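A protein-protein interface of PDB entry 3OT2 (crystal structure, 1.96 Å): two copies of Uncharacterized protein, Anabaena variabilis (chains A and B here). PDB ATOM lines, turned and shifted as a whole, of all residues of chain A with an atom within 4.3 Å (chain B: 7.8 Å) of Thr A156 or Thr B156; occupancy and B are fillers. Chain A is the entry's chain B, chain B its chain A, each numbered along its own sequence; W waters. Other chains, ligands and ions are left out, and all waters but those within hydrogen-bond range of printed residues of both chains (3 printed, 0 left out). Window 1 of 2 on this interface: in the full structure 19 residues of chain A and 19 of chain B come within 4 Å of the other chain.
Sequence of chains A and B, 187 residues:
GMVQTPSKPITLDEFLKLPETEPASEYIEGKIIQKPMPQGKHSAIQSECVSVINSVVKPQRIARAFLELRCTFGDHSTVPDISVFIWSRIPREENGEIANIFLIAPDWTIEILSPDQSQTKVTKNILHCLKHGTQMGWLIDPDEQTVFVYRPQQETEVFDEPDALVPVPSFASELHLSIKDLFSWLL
The side-chain hydroxyl (OG1) of Thr B156 lies within hydrogen-bond range of the side-chain hydroxyl (OG1) of Thr A156, at 3.0 Å.
N of Gln B153 lies within hydrogen-bond range of OE1 of Glu A155 (2.8 Å).
CD2 of Leu A127 touches OE2 of Glu B155, at 3.6 Å.
Leu A127 touches Thr B156 (CD1 to O, 3.8 Å).
Val B158 touches Leu A127.
CE1 of Phe A148 touches CG2 of Thr B123 (3.7 Å).
Gln A154 touches Gln B154 (C to C, 3.8 Å).
Gln A154 touches Glu B155.
OE2 of Glu A155 touches CD2 of Leu B127 (3.7 Å).
OE2 of Glu A155 touches CD1 of Leu B130 (3.96 Å).
CA of Glu A155 touches O of Gln B154, at 3.3 Å.
Glu A155 touches Glu B155.
Water W3 lies within hydrogen-bond range of the side-chain carboxylate (OE1) of Glu A155 and the side-chain amide nitrogen (NE2) of Gln B153.
Water W1 bridges OG1 of Thr B156 (2.7 Å) and N of Thr A156 (2.9 Å).
Water W2 lies within hydrogen-bond range of OG1 of Thr A156 (2.8 Å), N of Thr B156 (2.8 Å) and O of Gln A154 (3.4 Å).
Of chain B, only Leu B127 and Thr B156 come within 4 Å of Thr A156.
Printed residues of chain A within 4 Å of Leu B130: Glu A155.
Printed residues of chain A within 4 Å of Gln B154: Gln A154 and Glu A155.
Printed residues of chain A within 4 Å of Thr B123: Phe A148.
Leu B139 touches none of the printed residues of chain A.
The nearest residue of chain B that does not touch Thr A156 is Tyr B150 (4.6 Å).
Leu A127 touches Thr B156, and with the chains exchanged Thr A156 touches Leu B127.
Gln A154 touches its own counterpart, Gln B154.
Gln A154 touches Glu B155, and with the chains exchanged Glu A155 touches Gln B154.
Glu B155 touches its own counterpart, Glu A155.
Positions printed for both chains: 127, 148, 149, 150, 154, 155, 156 and 157.
Of the 13 pairs that touch across the chains among the printed residues, 9 have their exchanged pair printed and touching as well.
Of the 8 printed residues of chain A, 5 touch a printed residue of chain B.
Hydrophobic or aromatic side chains of chain A within 4 Å of the printed part of chain B: Leu A127 and Phe A148.
Of the 17 printed residues of chain B, 8 touch a printed residue of chain A.
Printed residues of chain B that touch a printed residue of chain A: Thr B123, Leu B127, Leu B130, Gln B153, Gln B154, Glu B155, Thr B156 and Val B158.
Hydrophobic or aromatic side chains of chain B within 4 Å of the printed part of chain A: Leu B127, Leu B130 and Val B158.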
ATOM      1  N   LEU A 127      18.751  26.657 -22.079  1.00  0.00           N
ATOM      2  CA  LEU A 127      19.112  25.436 -22.797  1.00  0.00           C
ATOM      3  C   LEU A 127      18.538  25.430 -24.232  1.00  0.00           C
ATOM      4  O   LEU A 127      19.199  24.903 -25.135  1.00  0.00           O
ATOM      5  CB  LEU A 127      18.713  24.172 -22.023  1.00  0.00           C
ATOM      6  CG  LEU A 127      19.445  23.995 -20.668  1.00  0.00           C
ATOM      7  CD1 LEU A 127      18.767  22.920 -19.821  1.00  0.00           C
ATOM      8  CD2 LEU A 127      20.940  23.728 -20.836  1.00  0.00           C
ATOM      9  N   PHE A 148      25.489  30.836 -12.818  1.00  0.00           N
ATOM     10  CA  PHE A 148      25.618  29.560 -13.529  1.00  0.00           C
ATOM     11  C   PHE A 148      25.967  29.885 -14.971  1.00  0.00           C
ATOM     12  O   PHE A 148      25.342  30.771 -15.577  1.00  0.00           O
ATOM     13  CB  PHE A 148      24.345  28.718 -13.466  1.00  0.00           C
ATOM     14  CG  PHE A 148      23.982  28.185 -12.104  1.00  0.00           C
ATOM     15  CD1 PHE A 148      24.713  27.160 -11.523  1.00  0.00           C
ATOM     16  CD2 PHE A 148      22.911  28.710 -11.400  1.00  0.00           C
ATOM     17  CE1 PHE A 148      24.349  26.630 -10.275  1.00  0.00           C
ATOM     18  CE2 PHE A 148      22.553  28.188 -10.142  1.00  0.00           C
ATOM     19  CZ  PHE A 148      23.275  27.147  -9.592  1.00  0.00           C
ATOM     20  N   VAL A 149      27.002  29.227 -15.493  1.00  0.00           N
ATOM     21  CA  VAL A 149      27.476  29.446 -16.862  1.00  0.00           C
ATOM     22  C   VAL A 149      27.139  28.204 -17.701  1.00  0.00           C
ATOM     23  O   VAL A 149      27.503  27.079 -17.337  1.00  0.00           O
ATOM     24  CB  VAL A 149      28.985  29.785 -16.896  1.00  0.00           C
ATOM     25  CG1 VAL A 149      29.530  29.728 -18.328  1.00  0.00           C
ATOM     26  CG2 VAL A 149      29.231  31.166 -16.286  1.00  0.00           C
ATOM     27  N   TYR A 150      26.447  28.437 -18.823  1.00  0.00           N
ATOM     28  CA  TYR A 150      25.995  27.419 -19.755  1.00  0.00           C
ATOM     29  C   TYR A 150      26.702  27.541 -21.113  1.00  0.00           C
ATOM     30  O   TYR A 150      26.627  28.590 -21.723  1.00  0.00           O
ATOM     31  CB  TYR A 150      24.481  27.580 -19.957  1.00  0.00           C
ATOM     32  CG  TYR A 150      23.663  27.261 -18.724  1.00  0.00           C
ATOM     33  CD1 TYR A 150      23.405  28.237 -17.758  1.00  0.00           C
ATOM     34  CD2 TYR A 150      23.100  26.004 -18.548  1.00  0.00           C
ATOM     35  CE1 TYR A 150      22.642  27.943 -16.620  1.00  0.00           C
ATOM     36  CE2 TYR A 150      22.351  25.697 -17.417  1.00  0.00           C
ATOM     37  CZ  TYR A 150      22.129  26.667 -16.452  1.00  0.00           C
ATOM     38  OH  TYR A 150      21.392  26.322 -15.350  1.00  0.00           O
ATOM     39  N   GLN A 154      28.322  21.202 -22.666  1.00  0.00           N
ATOM     40  CA  GLN A 154      29.196  21.215 -21.493  1.00  0.00           C
ATOM     41  C   GLN A 154      28.351  21.217 -20.234  1.00  0.00           C
ATOM     42  O   GLN A 154      27.312  21.864 -20.212  1.00  0.00           O
ATOM     43  CB  GLN A 154      30.124  22.453 -21.518  1.00  0.00           C
ATOM     44  CG  GLN A 154      31.307  22.289 -22.494  1.00  0.00           C
ATOM     45  CD  GLN A 154      32.281  23.435 -22.448  1.00  0.00           C
ATOM     46  OE1 GLN A 154      32.625  24.017 -23.482  1.00  0.00           O
ATOM     47  NE2 GLN A 154      32.775  23.760 -21.257  1.00  0.00           N
ATOM     48  N   GLU A 155      28.824  20.526 -19.174  1.00  0.00           N
ATOM     49  CA  GLU A 155      28.190  20.537 -17.848  1.00  0.00           C
ATOM     50  C   GLU A 155      28.050  22.003 -17.385  1.00  0.00           C
ATOM     51  O   GLU A 155      28.931  22.817 -17.676  1.00  0.00           O
ATOM     52  CB  GLU A 155      29.105  19.752 -16.880  1.00  0.00           C
ATOM     53  CG  GLU A 155      28.597  19.583 -15.451  1.00  0.00           C
ATOM     54  CD  GLU A 155      29.504  18.705 -14.599  1.00  0.00           C
ATOM     55  OE1 GLU A 155      30.102  17.762 -15.163  1.00  0.00           O
ATOM     56  OE2 GLU A 155      29.636  18.971 -13.381  1.00  0.00           O
ATOM     57  N   THR A 156      26.972  22.335 -16.652  1.00  0.00           N
ATOM     58  CA  THR A 156      26.776  23.696 -16.127  1.00  0.00           C
ATOM     59  C   THR A 156      27.953  24.025 -15.202  1.00  0.00           C
ATOM     60  O   THR A 156      28.411  23.149 -14.486  1.00  0.00           O
ATOM     61  CB  THR A 156      25.423  23.759 -15.373  1.00  0.00           C
ATOM     62  OG1 THR A 156      24.361  23.338 -16.232  1.00  0.00           O
ATOM     63  CG2 THR A 156      25.112  25.155 -14.809  1.00  0.00           C
ATOM     64  N   GLU A 157      28.453  25.252 -15.240  1.00  0.00           N
ATOM     65  CA  GLU A 157      29.567  25.675 -14.377  1.00  0.00           C
ATOM     66  C   GLU A 157      29.070  26.668 -13.339  1.00  0.00           C
ATOM     67  O   GLU A 157      28.189  27.449 -13.649  1.00  0.00           O
ATOM     68  CB  GLU A 157      30.689  26.290 -15.200  1.00  0.00           C
ATOM     69  CG  GLU A 157      31.492  25.255 -15.944  1.00  0.00           C
ATOM     70  CD  GLU A 157      32.628  25.781 -16.795  1.00  0.00           C
ATOM     71  OE1 GLU A 157      32.795  27.017 -16.877  1.00  0.00           O
ATOM     72  OE2 GLU A 157      33.300  24.951 -17.446  1.00  0.00           O
ATOM     73  N   THR B 123      21.261  22.676  -7.201  1.00  0.00           N
ATOM     74  CA  THR B 123      22.025  22.528  -8.453  1.00  0.00           C
ATOM     75  C   THR B 123      23.515  22.448  -8.120  1.00  0.00           C
ATOM     76  O   THR B 123      24.183  21.554  -8.630  1.00  0.00           O
ATOM     77  CB  THR B 123      21.689  23.653  -9.438  1.00  0.00           C
ATOM     78  OG1 THR B 123      20.306  23.537  -9.714  1.00  0.00           O
ATOM     79  CG2 THR B 123      22.434  23.509 -10.735  1.00  0.00           C
ATOM     80  N   LEU B 127      25.974  19.301  -8.857  1.00  0.00           N
ATOM     81  CA  LEU B 127      27.209  19.455  -9.627  1.00  0.00           C
ATOM     82  C   LEU B 127      28.441  19.034  -8.808  1.00  0.00           C
ATOM     83  O   LEU B 127      29.380  18.486  -9.386  1.00  0.00           O
ATOM     84  CB  LEU B 127      27.341  20.876 -10.190  1.00  0.00           C
ATOM     85  CG  LEU B 127      26.245  21.276 -11.205  1.00  0.00           C
ATOM     86  CD1 LEU B 127      26.261  22.770 -11.449  1.00  0.00           C
ATOM     87  CD2 LEU B 127      26.359  20.491 -12.525  1.00  0.00           C
ATOM     88  N   LEU B 130      28.723  15.192  -9.036  1.00  0.00           N
ATOM     89  CA  LEU B 130      29.306  14.816 -10.327  1.00  0.00           C
ATOM     90  C   LEU B 130      30.819  15.009 -10.338  1.00  0.00           C
ATOM     91  O   LEU B 130      31.527  14.214 -10.956  1.00  0.00           O
ATOM     92  CB  LEU B 130      28.678  15.609 -11.483  1.00  0.00           C
ATOM     93  CG  LEU B 130      27.185  15.396 -11.751  1.00  0.00           C
ATOM     94  CD1 LEU B 130      26.683  16.413 -12.757  1.00  0.00           C
ATOM     95  CD2 LEU B 130      26.889  13.979 -12.243  1.00  0.00           C
ATOM     96  N   GLY B 137      22.652  12.774 -11.756  1.00  0.00           N
ATOM     97  CA  GLY B 137      21.852  13.589 -10.862  1.00  0.00           C
ATOM     98  C   GLY B 137      20.488  13.822 -11.475  1.00  0.00           C
ATOM     99  O   GLY B 137      20.372  13.993 -12.691  1.00  0.00           O
ATOM    100  N   LEU B 139      17.127  16.350 -10.830  1.00  0.00           N
ATOM    101  CA  LEU B 139      16.515  17.474 -10.132  1.00  0.00           C
ATOM    102  C   LEU B 139      15.053  17.457 -10.545  1.00  0.00           C
ATOM    103  O   LEU B 139      14.728  17.753 -11.699  1.00  0.00           O
ATOM    104  CB  LEU B 139      17.199  18.835 -10.404  1.00  0.00           C
ATOM    105  CG  LEU B 139      16.491  20.069  -9.795  1.00  0.00           C
ATOM    106  CD1 LEU B 139      16.205  19.888  -8.321  1.00  0.00           C
ATOM    107  CD2 LEU B 139      17.297  21.317 -10.016  1.00  0.00           C
ATOM    108  N   VAL B 147      11.893  17.163 -14.924  1.00  0.00           N
ATOM    109  CA  VAL B 147      13.086  16.544 -14.367  1.00  0.00           C
ATOM    110  C   VAL B 147      14.297  17.043 -15.161  1.00  0.00           C
ATOM    111  O   VAL B 147      14.323  16.923 -16.390  1.00  0.00           O
ATOM    112  CB  VAL B 147      13.057  14.994 -14.276  1.00  0.00           C
ATOM    113  CG1 VAL B 147      14.325  14.485 -13.589  1.00  0.00           C
ATOM    114  CG2 VAL B 147      11.811  14.510 -13.519  1.00  0.00           C
ATOM    115  N   PHE B 148      15.298  17.591 -14.453  1.00  0.00           N
ATOM    116  CA  PHE B 148      16.585  17.925 -15.060  1.00  0.00           C
ATOM    117  C   PHE B 148      17.499  16.762 -14.794  1.00  0.00           C
ATOM    118  O   PHE B 148      17.563  16.282 -13.653  1.00  0.00           O
ATOM    119  CB  PHE B 148      17.189  19.221 -14.506  1.00  0.00           C
ATOM    120  CG  PHE B 148      16.449  20.489 -14.851  1.00  0.00           C
ATOM    121  CD1 PHE B 148      16.474  20.998 -16.140  1.00  0.00           C
ATOM    122  CD2 PHE B 148      15.728  21.174 -13.883  1.00  0.00           C
ATOM    123  CE1 PHE B 148      15.810  22.195 -16.455  1.00  0.00           C
ATOM    124  CE2 PHE B 148      15.086  22.390 -14.194  1.00  0.00           C
ATOM    125  CZ  PHE B 148      15.136  22.884 -15.478  1.00  0.00           C
ATOM    126  N   VAL B 149      18.173  16.280 -15.831  1.00  0.00           N
ATOM    127  CA  VAL B 149      19.100  15.147 -15.744  1.00  0.00           C
ATOM    128  C   VAL B 149      20.527  15.671 -15.925  1.00  0.00           C
ATOM    129  O   VAL B 149      20.843  16.309 -16.935  1.00  0.00           O
ATOM    130  CB  VAL B 149      18.738  14.034 -16.759  1.00  0.00           C
ATOM    131  CG1 VAL B 149      19.855  12.984 -16.849  1.00  0.00           C
ATOM    132  CG2 VAL B 149      17.412  13.368 -16.385  1.00  0.00           C
ATOM    133  N   TYR B 150      21.386  15.359 -14.952  1.00  0.00           N
ATOM    134  CA  TYR B 150      22.779  15.767 -14.908  1.00  0.00           C
ATOM    135  C   TYR B 150      23.722  14.561 -15.040  1.00  0.00           C
ATOM    136  O   TYR B 150      23.611  13.634 -14.257  1.00  0.00           O
ATOM    137  CB  TYR B 150      23.045  16.462 -13.563  1.00  0.00           C
ATOM    138  CG  TYR B 150      22.332  17.781 -13.389  1.00  0.00           C
ATOM    139  CD1 TYR B 150      21.023  17.835 -12.913  1.00  0.00           C
ATOM    140  CD2 TYR B 150      22.972  18.981 -13.675  1.00  0.00           C
ATOM    141  CE1 TYR B 150      20.371  19.054 -12.733  1.00  0.00           C
ATOM    142  CE2 TYR B 150      22.326  20.206 -13.503  1.00  0.00           C
ATOM    143  CZ  TYR B 150      21.023  20.236 -13.045  1.00  0.00           C
ATOM    144  OH  TYR B 150      20.407  21.450 -12.889  1.00  0.00           O
ATOM    145  N   ARG B 151      24.636  14.595 -16.026  1.00  0.00           N
ATOM    146  CA  ARG B 151      25.648  13.564 -16.259  1.00  0.00           C
ATOM    147  C   ARG B 151      27.014  14.237 -16.303  1.00  0.00           C
ATOM    148  O   ARG B 151      27.084  15.412 -16.707  1.00  0.00           O
ATOM    149  CB  ARG B 151      25.383  12.799 -17.560  1.00  0.00           C
ATOM    150  CG  ARG B 151      24.129  11.934 -17.563  1.00  0.00           C
ATOM    151  CD  ARG B 151      23.980  11.411 -18.963  1.00  0.00           C
ATOM    152  NE  ARG B 151      23.101  10.265 -19.079  1.00  0.00           N
ATOM    153  CZ  ARG B 151      21.969  10.237 -19.782  1.00  0.00           C
ATOM    154  NH1 ARG B 151      21.522  11.336 -20.384  1.00  0.00           N
ATOM    155  NH2 ARG B 151      21.275   9.112 -19.888  1.00  0.00           N
ATOM    156  N   GLN B 153      30.278  15.981 -17.372  1.00  0.00           N
ATOM    157  CA  GLN B 153      30.773  16.641 -18.578  1.00  0.00           C
ATOM    158  C   GLN B 153      29.717  16.697 -19.705  1.00  0.00           C
ATOM    159  O   GLN B 153      30.070  16.815 -20.872  1.00  0.00           O
ATOM    160  CB  GLN B 153      32.069  15.963 -19.088  1.00  0.00           C
ATOM    161  CG  GLN B 153      33.327  16.331 -18.307  1.00  0.00           C
ATOM    162  CD  GLN B 153      33.442  15.558 -17.021  1.00  0.00           C
ATOM    163  OE1 GLN B 153      33.588  14.326 -17.010  1.00  0.00           O
ATOM    164  NE2 GLN B 153      33.360  16.268 -15.908  1.00  0.00           N
ATOM    165  N   GLN B 154      28.438  16.670 -19.356  1.00  0.00           N
ATOM    166  CA  GLN B 154      27.375  16.763 -20.364  1.00  0.00           C
ATOM    167  C   GLN B 154      26.449  17.899 -20.017  1.00  0.00           C
ATOM    168  O   GLN B 154      26.193  18.127 -18.845  1.00  0.00           O
ATOM    169  CB  GLN B 154      26.585  15.436 -20.436  1.00  0.00           C
ATOM    170  CG  GLN B 154      27.338  14.320 -21.182  1.00  0.00           C
ATOM    171  CD  GLN B 154      26.506  13.062 -21.358  1.00  0.00           C
ATOM    172  OE1 GLN B 154      26.946  11.948 -21.032  1.00  0.00           O
ATOM    173  NE2 GLN B 154      25.286  13.195 -21.897  1.00  0.00           N
ATOM    174  N   GLU B 155      25.909  18.593 -21.024  1.00  0.00           N
ATOM    175  CA  GLU B 155      24.918  19.657 -20.853  1.00  0.00           C
ATOM    176  C   GLU B 155      23.719  19.096 -20.101  1.00  0.00           C
ATOM    177  O   GLU B 155      23.388  17.914 -20.278  1.00  0.00           O
ATOM    178  CB  GLU B 155      24.484  20.157 -22.247  1.00  0.00           C
ATOM    179  CG  GLU B 155      23.575  21.364 -22.274  1.00  0.00           C
ATOM    180  CD  GLU B 155      23.340  21.901 -23.676  1.00  0.00           C
ATOM    181  OE1 GLU B 155      24.225  21.732 -24.547  1.00  0.00           O
ATOM    182  OE2 GLU B 155      22.265  22.500 -23.901  1.00  0.00           O
ATOM    183  N   THR B 156      23.084  19.914 -19.239  1.00  0.00           N
ATOM    184  CA  THR B 156      21.889  19.493 -18.489  1.00  0.00           C
ATOM    185  C   THR B 156      20.813  19.085 -19.501  1.00  0.00           C
ATOM    186  O   THR B 156      20.673  19.747 -20.538  1.00  0.00           O
ATOM    187  CB  THR B 156      21.405  20.646 -17.570  1.00  0.00           C
ATOM    188  OG1 THR B 156      22.476  21.062 -16.734  1.00  0.00           O
ATOM    189  CG2 THR B 156      20.194  20.259 -16.711  1.00  0.00           C
ATOM    190  N   GLU B 157      20.083  17.994 -19.223  1.00  0.00           N
ATOM    191  CA  GLU B 157      18.999  17.534 -20.117  1.00  0.00           C
ATOM    192  C   GLU B 157      17.662  17.764 -19.447  1.00  0.00           C
ATOM    193  O   GLU B 157      17.563  17.623 -18.231  1.00  0.00           O
ATOM    194  CB  GLU B 157      19.171  16.059 -20.466  1.00  0.00           C
ATOM    195  CG  GLU B 157      20.278  15.819 -21.465  1.00  0.00           C
ATOM    196  CD  GLU B 157      20.521  14.373 -21.848  1.00  0.00           C
ATOM    197  OE1 GLU B 157      19.838  13.478 -21.299  1.00  0.00           O
ATOM    198  OE2 GLU B 157      21.446  14.130 -22.655  1.00  0.00           O
ATOM    199  N   VAL B 158      16.644  18.135 -20.222  1.00  0.00           N
ATOM    200  CA  VAL B 158      15.308  18.474 -19.709  1.00  0.00           C
ATOM    201  C   VAL B 158      14.297  17.433 -20.144  1.00  0.00           C
ATOM    202  O   VAL B 158      14.206  17.139 -21.341  1.00  0.00           O
ATOM    203  CB  VAL B 158      14.824  19.882 -20.183  1.00  0.00           C
ATOM    204  CG1 VAL B 158      13.594  20.327 -19.405  1.00  0.00           C
ATOM    205  CG2 VAL B 158      15.907  20.920 -20.056  1.00  0.00           C
ATOM    206  N   PHE B 159      13.473  16.959 -19.201  1.00  0.00           N
ATOM    207  CA  PHE B 159      12.380  16.012 -19.478  1.00  0.00           C
ATOM    208  C   PHE B 159      11.095  16.596 -18.908  1.00  0.00           C
ATOM    209  O   PHE B 159      11.030  16.883 -17.707  1.00  0.00           O
ATOM    210  CB  PHE B 159      12.718  14.605 -18.891  1.00  0.00           C
ATOM    211  CG  PHE B 159      13.917  14.032 -19.623  1.00  0.00           C
ATOM    212  CD1 PHE B 159      13.758  13.369 -20.839  1.00  0.00           C
ATOM    213  CD2 PHE B 159      15.213  14.294 -19.182  1.00  0.00           C
ATOM    214  CE1 PHE B 159      14.870  12.940 -21.566  1.00  0.00           C
ATOM    215  CE2 PHE B 159      16.317  13.895 -19.927  1.00  0.00           C
ATOM    216  CZ  PHE B 159      16.139  13.233 -21.124  1.00  0.00           C
HETATM  217  O   HOH W   1      25.025  20.242 -16.215  1.00  0.00           O
HETATM  218  O   HOH W   2      24.252  22.486 -18.910  1.00  0.00           O
HETATM  219  O   HOH W   3      31.872  16.833 -13.387  1.00  0.00           O
